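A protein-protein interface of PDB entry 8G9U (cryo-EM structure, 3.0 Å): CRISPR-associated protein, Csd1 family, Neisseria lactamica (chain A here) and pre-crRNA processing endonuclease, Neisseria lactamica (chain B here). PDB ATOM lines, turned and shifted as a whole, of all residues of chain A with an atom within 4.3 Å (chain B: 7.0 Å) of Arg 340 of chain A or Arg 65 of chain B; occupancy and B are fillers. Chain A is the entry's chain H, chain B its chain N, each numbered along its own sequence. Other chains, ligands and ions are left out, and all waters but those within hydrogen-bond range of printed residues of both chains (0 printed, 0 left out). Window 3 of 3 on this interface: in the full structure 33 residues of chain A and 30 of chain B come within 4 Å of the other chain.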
ATOM      1  N   VAL A 269      26.812   0.633  -7.168  1.00  0.00           N
ATOM      2  CA  VAL A 269      25.878  -0.301  -7.783  1.00  0.00           C
ATOM      3  C   VAL A 269      26.257  -1.747  -7.474  1.00  0.00           C
ATOM      4  O   VAL A 269      27.078  -2.361  -8.160  1.00  0.00           O
ATOM      5  CB  VAL A 269      25.768  -0.010  -9.293  1.00  0.00           C
ATOM      6  CG1 VAL A 269      27.087  -0.168  -9.977  1.00  0.00           C
ATOM      7  CG2 VAL A 269      24.779  -0.943  -9.922  1.00  0.00           C
ATOM      8  N   GLY A 329      24.367  -6.265 -12.500  1.00  0.00           N
ATOM      9  CA  GLY A 329      24.638  -5.107 -11.683  1.00  0.00           C
ATOM     10  C   GLY A 329      23.385  -4.457 -11.151  1.00  0.00           C
ATOM     11  O   GLY A 329      23.142  -3.275 -11.382  1.00  0.00           O
ATOM     12  N   LEU A 330      22.581  -5.228 -10.438  1.00  0.00           N
ATOM     13  CA  LEU A 330      21.398  -4.705  -9.776  1.00  0.00           C
ATOM     14  C   LEU A 330      21.660  -3.499  -8.881  1.00  0.00           C
ATOM     15  O   LEU A 330      22.804  -3.202  -8.542  1.00  0.00           O
ATOM     16  CB  LEU A 330      20.752  -5.838  -8.996  1.00  0.00           C
ATOM     17  CG  LEU A 330      21.689  -6.415  -7.947  1.00  0.00           C
ATOM     18  CD1 LEU A 330      21.759  -5.680  -6.654  1.00  0.00           C
ATOM     19  CD2 LEU A 330      21.201  -7.790  -7.675  1.00  0.00           C
ATOM     20  N   SER A 331      20.599  -2.783  -8.518  1.00  0.00           N
ATOM     21  CA  SER A 331      20.684  -1.687  -7.568  1.00  0.00           C
ATOM     22  C   SER A 331      19.282  -1.387  -7.077  1.00  0.00           C
ATOM     23  O   SER A 331      18.318  -1.597  -7.816  1.00  0.00           O
ATOM     24  CB  SER A 331      21.300  -0.439  -8.202  1.00  0.00           C
ATOM     25  OG  SER A 331      20.318   0.292  -8.909  1.00  0.00           O
ATOM     26  N   ASN A 333      15.773   0.331  -6.149  1.00  0.00           N
ATOM     27  CA  ASN A 333      15.035   1.514  -6.557  1.00  0.00           C
ATOM     28  C   ASN A 333      14.451   2.203  -5.334  1.00  0.00           C
ATOM     29  O   ASN A 333      14.940   3.259  -4.923  1.00  0.00           O
ATOM     30  CB  ASN A 333      13.929   1.139  -7.530  1.00  0.00           C
ATOM     31  CG  ASN A 333      13.395   2.324  -8.274  1.00  0.00           C
ATOM     32  OD1 ASN A 333      13.686   3.466  -7.934  1.00  0.00           O
ATOM     33  ND2 ASN A 333      12.613   2.066  -9.308  1.00  0.00           N
ATOM     34  N   VAL A 338      16.679  -2.597  -9.488  1.00  0.00           N
ATOM     35  CA  VAL A 338      16.964  -2.049 -10.802  1.00  0.00           C
ATOM     36  C   VAL A 338      18.176  -2.781 -11.346  1.00  0.00           C
ATOM     37  O   VAL A 338      19.277  -2.644 -10.815  1.00  0.00           O
ATOM     38  CB  VAL A 338      17.234  -0.545 -10.727  1.00  0.00           C
ATOM     39  CG1 VAL A 338      17.857  -0.074 -12.010  1.00  0.00           C
ATOM     40  CG2 VAL A 338      15.972   0.205 -10.430  1.00  0.00           C
ATOM     41  N   VAL A 339      17.989  -3.542 -12.411  1.00  0.00           N
ATOM     42  CA  VAL A 339      19.126  -4.162 -13.067  1.00  0.00           C
ATOM     43  C   VAL A 339      19.863  -3.071 -13.816  1.00  0.00           C
ATOM     44  O   VAL A 339      19.450  -2.681 -14.910  1.00  0.00           O
ATOM     45  CB  VAL A 339      18.682  -5.277 -14.021  1.00  0.00           C
ATOM     46  CG1 VAL A 339      19.875  -5.896 -14.675  1.00  0.00           C
ATOM     47  CG2 VAL A 339      17.912  -6.306 -13.271  1.00  0.00           C
ATOM     48  N   ARG A 340      20.936  -2.546 -13.232  1.00  0.00           N
ATOM     49  CA  ARG A 340      21.684  -1.519 -13.942  1.00  0.00           C
ATOM     50  C   ARG A 340      22.681  -2.107 -14.921  1.00  0.00           C
ATOM     51  O   ARG A 340      22.902  -1.533 -15.990  1.00  0.00           O
ATOM     52  CB  ARG A 340      22.398  -0.594 -12.968  1.00  0.00           C
ATOM     53  CG  ARG A 340      21.454   0.231 -12.168  1.00  0.00           C
ATOM     54  CD  ARG A 340      22.182   1.161 -11.254  1.00  0.00           C
ATOM     55  NE  ARG A 340      21.231   1.883 -10.427  1.00  0.00           N
ATOM     56  CZ  ARG A 340      20.670   3.030 -10.782  1.00  0.00           C
ATOM     57  NH1 ARG A 340      19.808   3.630  -9.973  1.00  0.00           N
ATOM     58  NH2 ARG A 340      20.961   3.572 -11.956  1.00  0.00           N
ATOM     59  N   PHE A 341      23.296  -3.227 -14.584  1.00  0.00           N
ATOM     60  CA  PHE A 341      24.176  -3.923 -15.499  1.00  0.00           C
ATOM     61  C   PHE A 341      23.604  -5.289 -15.785  1.00  0.00           C
ATOM     62  O   PHE A 341      23.028  -5.930 -14.907  1.00  0.00           O
ATOM     63  CB  PHE A 341      25.574  -4.109 -14.941  1.00  0.00           C
ATOM     64  CG  PHE A 341      26.196  -2.858 -14.478  1.00  0.00           C
ATOM     65  CD1 PHE A 341      26.132  -1.718 -15.254  1.00  0.00           C
ATOM     66  CD2 PHE A 341      26.866  -2.816 -13.283  1.00  0.00           C
ATOM     67  CE1 PHE A 341      26.712  -0.546 -14.832  1.00  0.00           C
ATOM     68  CE2 PHE A 341      27.446  -1.656 -12.862  1.00  0.00           C
ATOM     69  CZ  PHE A 341      27.373  -0.515 -13.631  1.00  0.00           C
ATOM     70  N   GLU B  21      10.973  -2.321 -13.618  1.00  0.00           N
ATOM     71  CA  GLU B  21      12.312  -1.757 -13.694  1.00  0.00           C
ATOM     72  C   GLU B  21      12.873  -1.975 -15.079  1.00  0.00           C
ATOM     73  O   GLU B  21      13.973  -2.499 -15.254  1.00  0.00           O
ATOM     74  CB  GLU B  21      13.227  -2.348 -12.634  1.00  0.00           C
ATOM     75  CG  GLU B  21      12.918  -1.882 -11.227  1.00  0.00           C
ATOM     76  CD  GLU B  21      12.564  -0.409 -11.147  1.00  0.00           C
ATOM     77  OE1 GLU B  21      11.614  -0.070 -10.416  1.00  0.00           O
ATOM     78  OE2 GLU B  21      13.234   0.418 -11.792  1.00  0.00           O
ATOM     79  N   VAL B  23      13.712  -3.688 -18.231  1.00  0.00           N
ATOM     80  CA  VAL B  23      14.923  -4.165 -18.871  1.00  0.00           C
ATOM     81  C   VAL B  23      14.488  -4.758 -20.188  1.00  0.00           C
ATOM     82  O   VAL B  23      13.749  -5.746 -20.211  1.00  0.00           O
ATOM     83  CB  VAL B  23      15.666  -5.195 -18.017  1.00  0.00           C
ATOM     84  CG1 VAL B  23      16.914  -5.642 -18.723  1.00  0.00           C
ATOM     85  CG2 VAL B  23      16.021  -4.591 -16.689  1.00  0.00           C
ATOM     86  N   TRP B  61      22.926  -1.223 -24.598  1.00  0.00           N
ATOM     87  CA  TRP B  61      21.952  -0.822 -23.595  1.00  0.00           C
ATOM     88  C   TRP B  61      22.247   0.571 -23.063  1.00  0.00           C
ATOM     89  O   TRP B  61      23.402   0.985 -22.961  1.00  0.00           O
ATOM     90  CB  TRP B  61      21.936  -1.787 -22.417  1.00  0.00           C
ATOM     91  CG  TRP B  61      21.877  -3.207 -22.784  1.00  0.00           C
ATOM     92  CD1 TRP B  61      22.924  -4.022 -23.061  1.00  0.00           C
ATOM     93  CD2 TRP B  61      20.707  -4.005 -22.888  1.00  0.00           C
ATOM     94  NE1 TRP B  61      22.478  -5.284 -23.343  1.00  0.00           N
ATOM     95  CE2 TRP B  61      21.113  -5.296 -23.241  1.00  0.00           C
ATOM     96  CE3 TRP B  61      19.352  -3.751 -22.722  1.00  0.00           C
ATOM     97  CZ2 TRP B  61      20.216  -6.327 -23.426  1.00  0.00           C
ATOM     98  CZ3 TRP B  61      18.469  -4.771 -22.904  1.00  0.00           C
ATOM     99  CH2 TRP B  61      18.898  -6.042 -23.255  1.00  0.00           C
ATOM    100  N   THR B  62      21.178   1.289 -22.726  1.00  0.00           N
ATOM    101  CA  THR B  62      21.252   2.532 -21.969  1.00  0.00           C
ATOM    102  C   THR B  62      20.149   2.566 -20.930  1.00  0.00           C
ATOM    103  O   THR B  62      18.969   2.563 -21.280  1.00  0.00           O
ATOM    104  CB  THR B  62      21.124   3.770 -22.854  1.00  0.00           C
ATOM    105  OG1 THR B  62      19.752   3.955 -23.215  1.00  0.00           O
ATOM    106  CG2 THR B  62      21.991   3.678 -24.080  1.00  0.00           C
ATOM    107  N   ASN B  63      20.531   2.633 -19.664  1.00  0.00           N
ATOM    108  CA  ASN B  63      19.570   2.693 -18.576  1.00  0.00           C
ATOM    109  C   ASN B  63      18.974   4.091 -18.491  1.00  0.00           C
ATOM    110  O   ASN B  63      19.705   5.083 -18.516  1.00  0.00           O
ATOM    111  CB  ASN B  63      20.238   2.318 -17.258  1.00  0.00           C
ATOM    112  CG  ASN B  63      21.110   1.098 -17.386  1.00  0.00           C
ATOM    113  OD1 ASN B  63      20.660  -0.025 -17.175  1.00  0.00           O
ATOM    114  ND2 ASN B  63      22.371   1.307 -17.739  1.00  0.00           N
ATOM    115  N   ILE B  64      17.650   4.160 -18.375  1.00  0.00           N
ATOM    116  CA  ILE B  64      16.894   5.409 -18.325  1.00  0.00           C
ATOM    117  C   ILE B  64      15.820   5.272 -17.255  1.00  0.00           C
ATOM    118  O   ILE B  64      14.791   4.635 -17.494  1.00  0.00           O
ATOM    119  CB  ILE B  64      16.259   5.745 -19.682  1.00  0.00           C
ATOM    120  CG1 ILE B  64      17.317   5.892 -20.772  1.00  0.00           C
ATOM    121  CG2 ILE B  64      15.425   6.989 -19.600  1.00  0.00           C
ATOM    122  CD1 ILE B  64      18.307   7.005 -20.519  1.00  0.00           C
ATOM    123  N   ARG B  65      16.041   5.867 -16.084  1.00  0.00           N
ATOM    124  CA  ARG B  65      14.975   5.908 -15.082  1.00  0.00           C
ATOM    125  C   ARG B  65      14.033   7.034 -15.449  1.00  0.00           C
ATOM    126  O   ARG B  65      14.390   8.207 -15.428  1.00  0.00           O
ATOM    127  CB  ARG B  65      15.497   6.080 -13.663  1.00  0.00           C
ATOM    128  CG  ARG B  65      16.033   4.821 -13.062  1.00  0.00           C
ATOM    129  CD  ARG B  65      16.548   5.008 -11.669  1.00  0.00           C
ATOM    130  NE  ARG B  65      15.491   5.367 -10.740  1.00  0.00           N
ATOM    131  CZ  ARG B  65      15.716   5.719  -9.483  1.00  0.00           C
ATOM    132  NH1 ARG B  65      16.955   5.762  -9.021  1.00  0.00           N
ATOM    133  NH2 ARG B  65      14.707   6.023  -8.688  1.00  0.00           N
ATOM    134  N   ARG B  66      12.813   6.670 -15.798  1.00  0.00           N
ATOM    135  CA  ARG B  66      11.786   7.663 -16.010  1.00  0.00           C
ATOM    136  C   ARG B  66      10.839   7.662 -14.828  1.00  0.00           C
ATOM    137  O   ARG B  66      10.487   6.603 -14.299  1.00  0.00           O
ATOM    138  CB  ARG B  66      11.021   7.365 -17.289  1.00  0.00           C
ATOM    139  CG  ARG B  66      11.768   7.683 -18.538  1.00  0.00           C
ATOM    140  CD  ARG B  66      10.928   7.408 -19.768  1.00  0.00           C
ATOM    141  NE  ARG B  66      10.257   6.115 -19.727  1.00  0.00           N
ATOM    142  CZ  ARG B  66      10.772   4.994 -20.217  1.00  0.00           C
ATOM    143  NH1 ARG B  66      10.093   3.862 -20.137  1.00  0.00           N
ATOM    144  NH2 ARG B  66      11.964   5.003 -20.786  1.00  0.00           N
ATOM    145  N   ASN B  67      10.426   8.851 -14.405  1.00  0.00           N
ATOM    146  CA  ASN B  67       9.399   8.906 -13.384  1.00  0.00           C
ATOM    147  C   ASN B  67       8.083   8.507 -14.000  1.00  0.00           C
ATOM    148  O   ASN B  67       7.300   9.344 -14.451  1.00  0.00           O
ATOM    149  CB  ASN B  67       9.284  10.276 -12.765  1.00  0.00           C
ATOM    150  CG  ASN B  67      10.512  10.670 -12.046  1.00  0.00           C
ATOM    151  OD1 ASN B  67      11.189  11.606 -12.432  1.00  0.00           O
ATOM    152  ND2 ASN B  67      10.828   9.946 -10.992  1.00  0.00           N
ATOM    153  N   GLU B  68       7.845   7.219 -14.005  1.00  0.00           N
ATOM    154  CA  GLU B  68       6.665   6.663 -14.617  1.00  0.00           C
ATOM    155  C   GLU B  68       5.545   6.889 -13.599  1.00  0.00           C
ATOM    156  O   GLU B  68       5.791   7.314 -12.466  1.00  0.00           O
ATOM    157  CB  GLU B  68       6.934   5.199 -14.923  1.00  0.00           C
ATOM    158  CG  GLU B  68       8.066   4.910 -15.965  1.00  0.00           C
ATOM    159  CD  GLU B  68       7.854   5.338 -17.397  1.00  0.00           C
ATOM    160  OE1 GLU B  68       6.732   5.354 -17.878  1.00  0.00           O
ATOM    161  OE2 GLU B  68       8.846   5.591 -18.092  1.00  0.00           O
ATOM    162  N   GLN B  87       6.166   6.737  -9.559  1.00  0.00           N
ATOM    163  CA  GLN B  87       7.103   5.633  -9.478  1.00  0.00           C
ATOM    164  C   GLN B  87       8.288   5.988 -10.346  1.00  0.00           C
ATOM    165  O   GLN B  87       8.165   6.792 -11.259  1.00  0.00           O
ATOM    166  CB  GLN B  87       6.501   4.326  -9.950  1.00  0.00           C
ATOM    167  CG  GLN B  87       5.377   3.887  -9.102  1.00  0.00           C
ATOM    168  CD  GLN B  87       5.834   3.501  -7.735  1.00  0.00           C
ATOM    169  OE1 GLN B  87       5.152   3.753  -6.747  1.00  0.00           O
ATOM    170  NE2 GLN B  87       6.986   2.863  -7.664  1.00  0.00           N
ATOM    171  N   GLN B  88       9.440   5.407 -10.060  1.00  0.00           N
ATOM    172  CA  GLN B  88      10.623   5.672 -10.864  1.00  0.00           C
ATOM    173  C   GLN B  88      11.032   4.364 -11.517  1.00  0.00           C
ATOM    174  O   GLN B  88      11.821   3.595 -10.977  1.00  0.00           O
ATOM    175  CB  GLN B  88      11.703   6.242 -10.042  1.00  0.00           C
ATOM    176  CG  GLN B  88      11.217   7.292  -9.110  1.00  0.00           C
ATOM    177  CD  GLN B  88      12.272   8.307  -8.816  1.00  0.00           C
ATOM    178  OE1 GLN B  88      12.406   9.290  -9.526  1.00  0.00           O
ATOM    179  NE2 GLN B  88      13.025   8.085  -7.755  1.00  0.00           N
ATOM    180  N   ARG B  89      10.486   4.112 -12.694  1.00  0.00           N
ATOM    181  CA  ARG B  89      10.810   2.876 -13.381  1.00  0.00           C
ATOM    182  C   ARG B  89      12.118   3.078 -14.118  1.00  0.00           C
ATOM    183  O   ARG B  89      12.217   3.939 -14.995  1.00  0.00           O
ATOM    184  CB  ARG B  89       9.705   2.469 -14.343  1.00  0.00           C
ATOM    185  CG  ARG B  89       8.418   2.119 -13.674  1.00  0.00           C
ATOM    186  CD  ARG B  89       7.369   1.806 -14.702  1.00  0.00           C
ATOM    187  NE  ARG B  89       7.580   0.540 -15.372  1.00  0.00           N
ATOM    188  CZ  ARG B  89       6.677  -0.026 -16.156  1.00  0.00           C
ATOM    189  NH1 ARG B  89       5.513   0.570 -16.352  1.00  0.00           N
ATOM    190  NH2 ARG B  89       6.932  -1.185 -16.736  1.00  0.00           N
ATOM    191  N   ALA B  90      13.133   2.315 -13.741  1.00  0.00           N
ATOM    192  CA  ALA B  90      14.324   2.260 -14.560  1.00  0.00           C
ATOM    193  C   ALA B  90      13.989   1.619 -15.889  1.00  0.00           C
ATOM    194  O   ALA B  90      13.049   0.830 -16.002  1.00  0.00           O
ATOM    195  CB  ALA B  90      15.422   1.470 -13.870  1.00  0.00           C
ATOM    196  N   SER B  91      14.752   1.971 -16.909  1.00  0.00           N
ATOM    197  CA  SER B  91      14.562   1.367 -18.217  1.00  0.00           C
ATOM    198  C   SER B  91      15.932   1.052 -18.785  1.00  0.00           C
ATOM    199  O   SER B  91      16.618   1.946 -19.283  1.00  0.00           O
ATOM    200  CB  SER B  91      13.769   2.279 -19.146  1.00  0.00           C
ATOM    201  OG  SER B  91      12.429   2.397 -18.705  1.00  0.00           O
ATOM    202  N   MET B  92      16.341  -0.207 -18.694  1.00  0.00           N
ATOM    203  CA  MET B  92      17.497  -0.654 -19.458  1.00  0.00           C
ATOM    204  C   MET B  92      17.025  -0.759 -20.894  1.00  0.00           C
ATOM    205  O   MET B  92      16.488  -1.775 -21.329  1.00  0.00           O
ATOM    206  CB  MET B  92      18.048  -1.972 -18.943  1.00  0.00           C
ATOM    207  CG  MET B  92      19.316  -2.371 -19.663  1.00  0.00           C
ATOM    208  SD  MET B  92      20.064  -3.909 -19.129  1.00  0.00           S
ATOM    209  CE  MET B  92      20.703  -3.409 -17.553  1.00  0.00           C
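NH2 of Arg 65 of chain B lies within hydrogen-bond range of OD1 of Asn 333 of chain A, 2.9 Å away.
O of Arg 340 of chain A lies close to OD1 of Asn 63 of chain B, 3.0 Å away.
The side-chain amide nitrogen of Asn 333 of chain A lies within hydrogen-bond range of the side-chain carboxylate of Glu 21 of chain B (2.6 Å).
The side-chain amide nitrogen (ND2) of Asn 333 of chain A lies close to the backbone carbonyl oxygen (O) of Gln 88 of chain B.
The guanidinium group (NH2) of Arg 65 of chain B sits close to the side-chain amide nitrogen (NE2) of Gln 88 of chain B.
The backbone NH (N) of Arg 340 of chain A sits at hydrogen-bond distance from the backbone carbonyl oxygen (O) of Gly 329 of chain A, at 3.0 Å.
The backbone carbonyl oxygen of Ser 331 of chain A lies within hydrogen-bond range of the backbone NH of Val 338 of chain A (2.5 Å).
The side-chain carboxylate of Glu 21 of chain B lies within hydrogen-bond range of the backbone NH of Ala 90 of chain B, 2.7 Å away.
N of Gly 329 of chain A is in hydrogen-bond range of O of Phe 341 of chain A (2.8 Å).
CG2 of Val 338 of chain A touches OE2 of Glu 21 of chain B, at 3.1 Å.
Val 338 of chain A touches Ala 90 of chain B (CG1 to CB, 3.4 Å).
Val 23 of chain B touches Val 339 of chain A (CG2 to CB, 3.8 Å).
Asn 63 of chain B touches Val 339 of chain A (OD1 to O, 3.7 Å).
Val 339 of chain A touches Met 92 of chain B.
NH1 of Arg 340 of chain A touches NH1 of Arg 65 of chain B (3.7 Å).
CE of Met 92 of chain B touches O of Arg 340 of chain A, 3.3 Å away.
Met 92 of chain B touches Phe 341 of chain A.
Of chain B, only Asn 63, Arg 65 and Met 92 come within 4 Å of Arg 340 of chain A.
Arg 65 of chain B touches two residues of chain A.
Of the printed residues of chain B, Phe 341 of chain A touches Met 92 (3.9 Å).
Of the printed residues of chain A, Gln 88 of chain B touches Asn 333 (2.4 Å).
Of the printed residues of chain B, Val 338 of chain A touches Glu 21 (3.1 Å) and Ala 90 (3.4 Å).
Of the printed residues of chain A, Glu 21 of chain B touches Asn 333 and Val 338.
Asn 67 of chain B touches none of the printed residues of chain A.
The nearest residue of chain B that does not touch Arg 340 of chain A is Ala 90 of chain B (6.2 Å).
The nearest printed residue of chain A that does not touch Val 23 of chain B is Val 338 of chain A (6.0 Å).
Printed residues of chain B that touch a printed residue of chain A: Glu 21, Val 23, Asn 63, Arg 65, Gln 88, Ala 90 and Met 92.
Hydrophobic or aromatic side chains of chain B within 4 Å of the printed part of chain A: Val 23, Ala 90 and Met 92.
Printed residues of chain A that touch a printed residue of chain B: Asn 333, Val 338, Val 339, Arg 340 and Phe 341.
Hydrophobic or aromatic side chains of chain A that line the printed part of chain B: Val 338 and Val 339.
Among the printed residues, 12 pairs touch across the chains.
Among the printed residues, no Asp or Glu carboxylate lies within 4 Å of a Lys or Arg side-chain nitrogen of the other chain.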
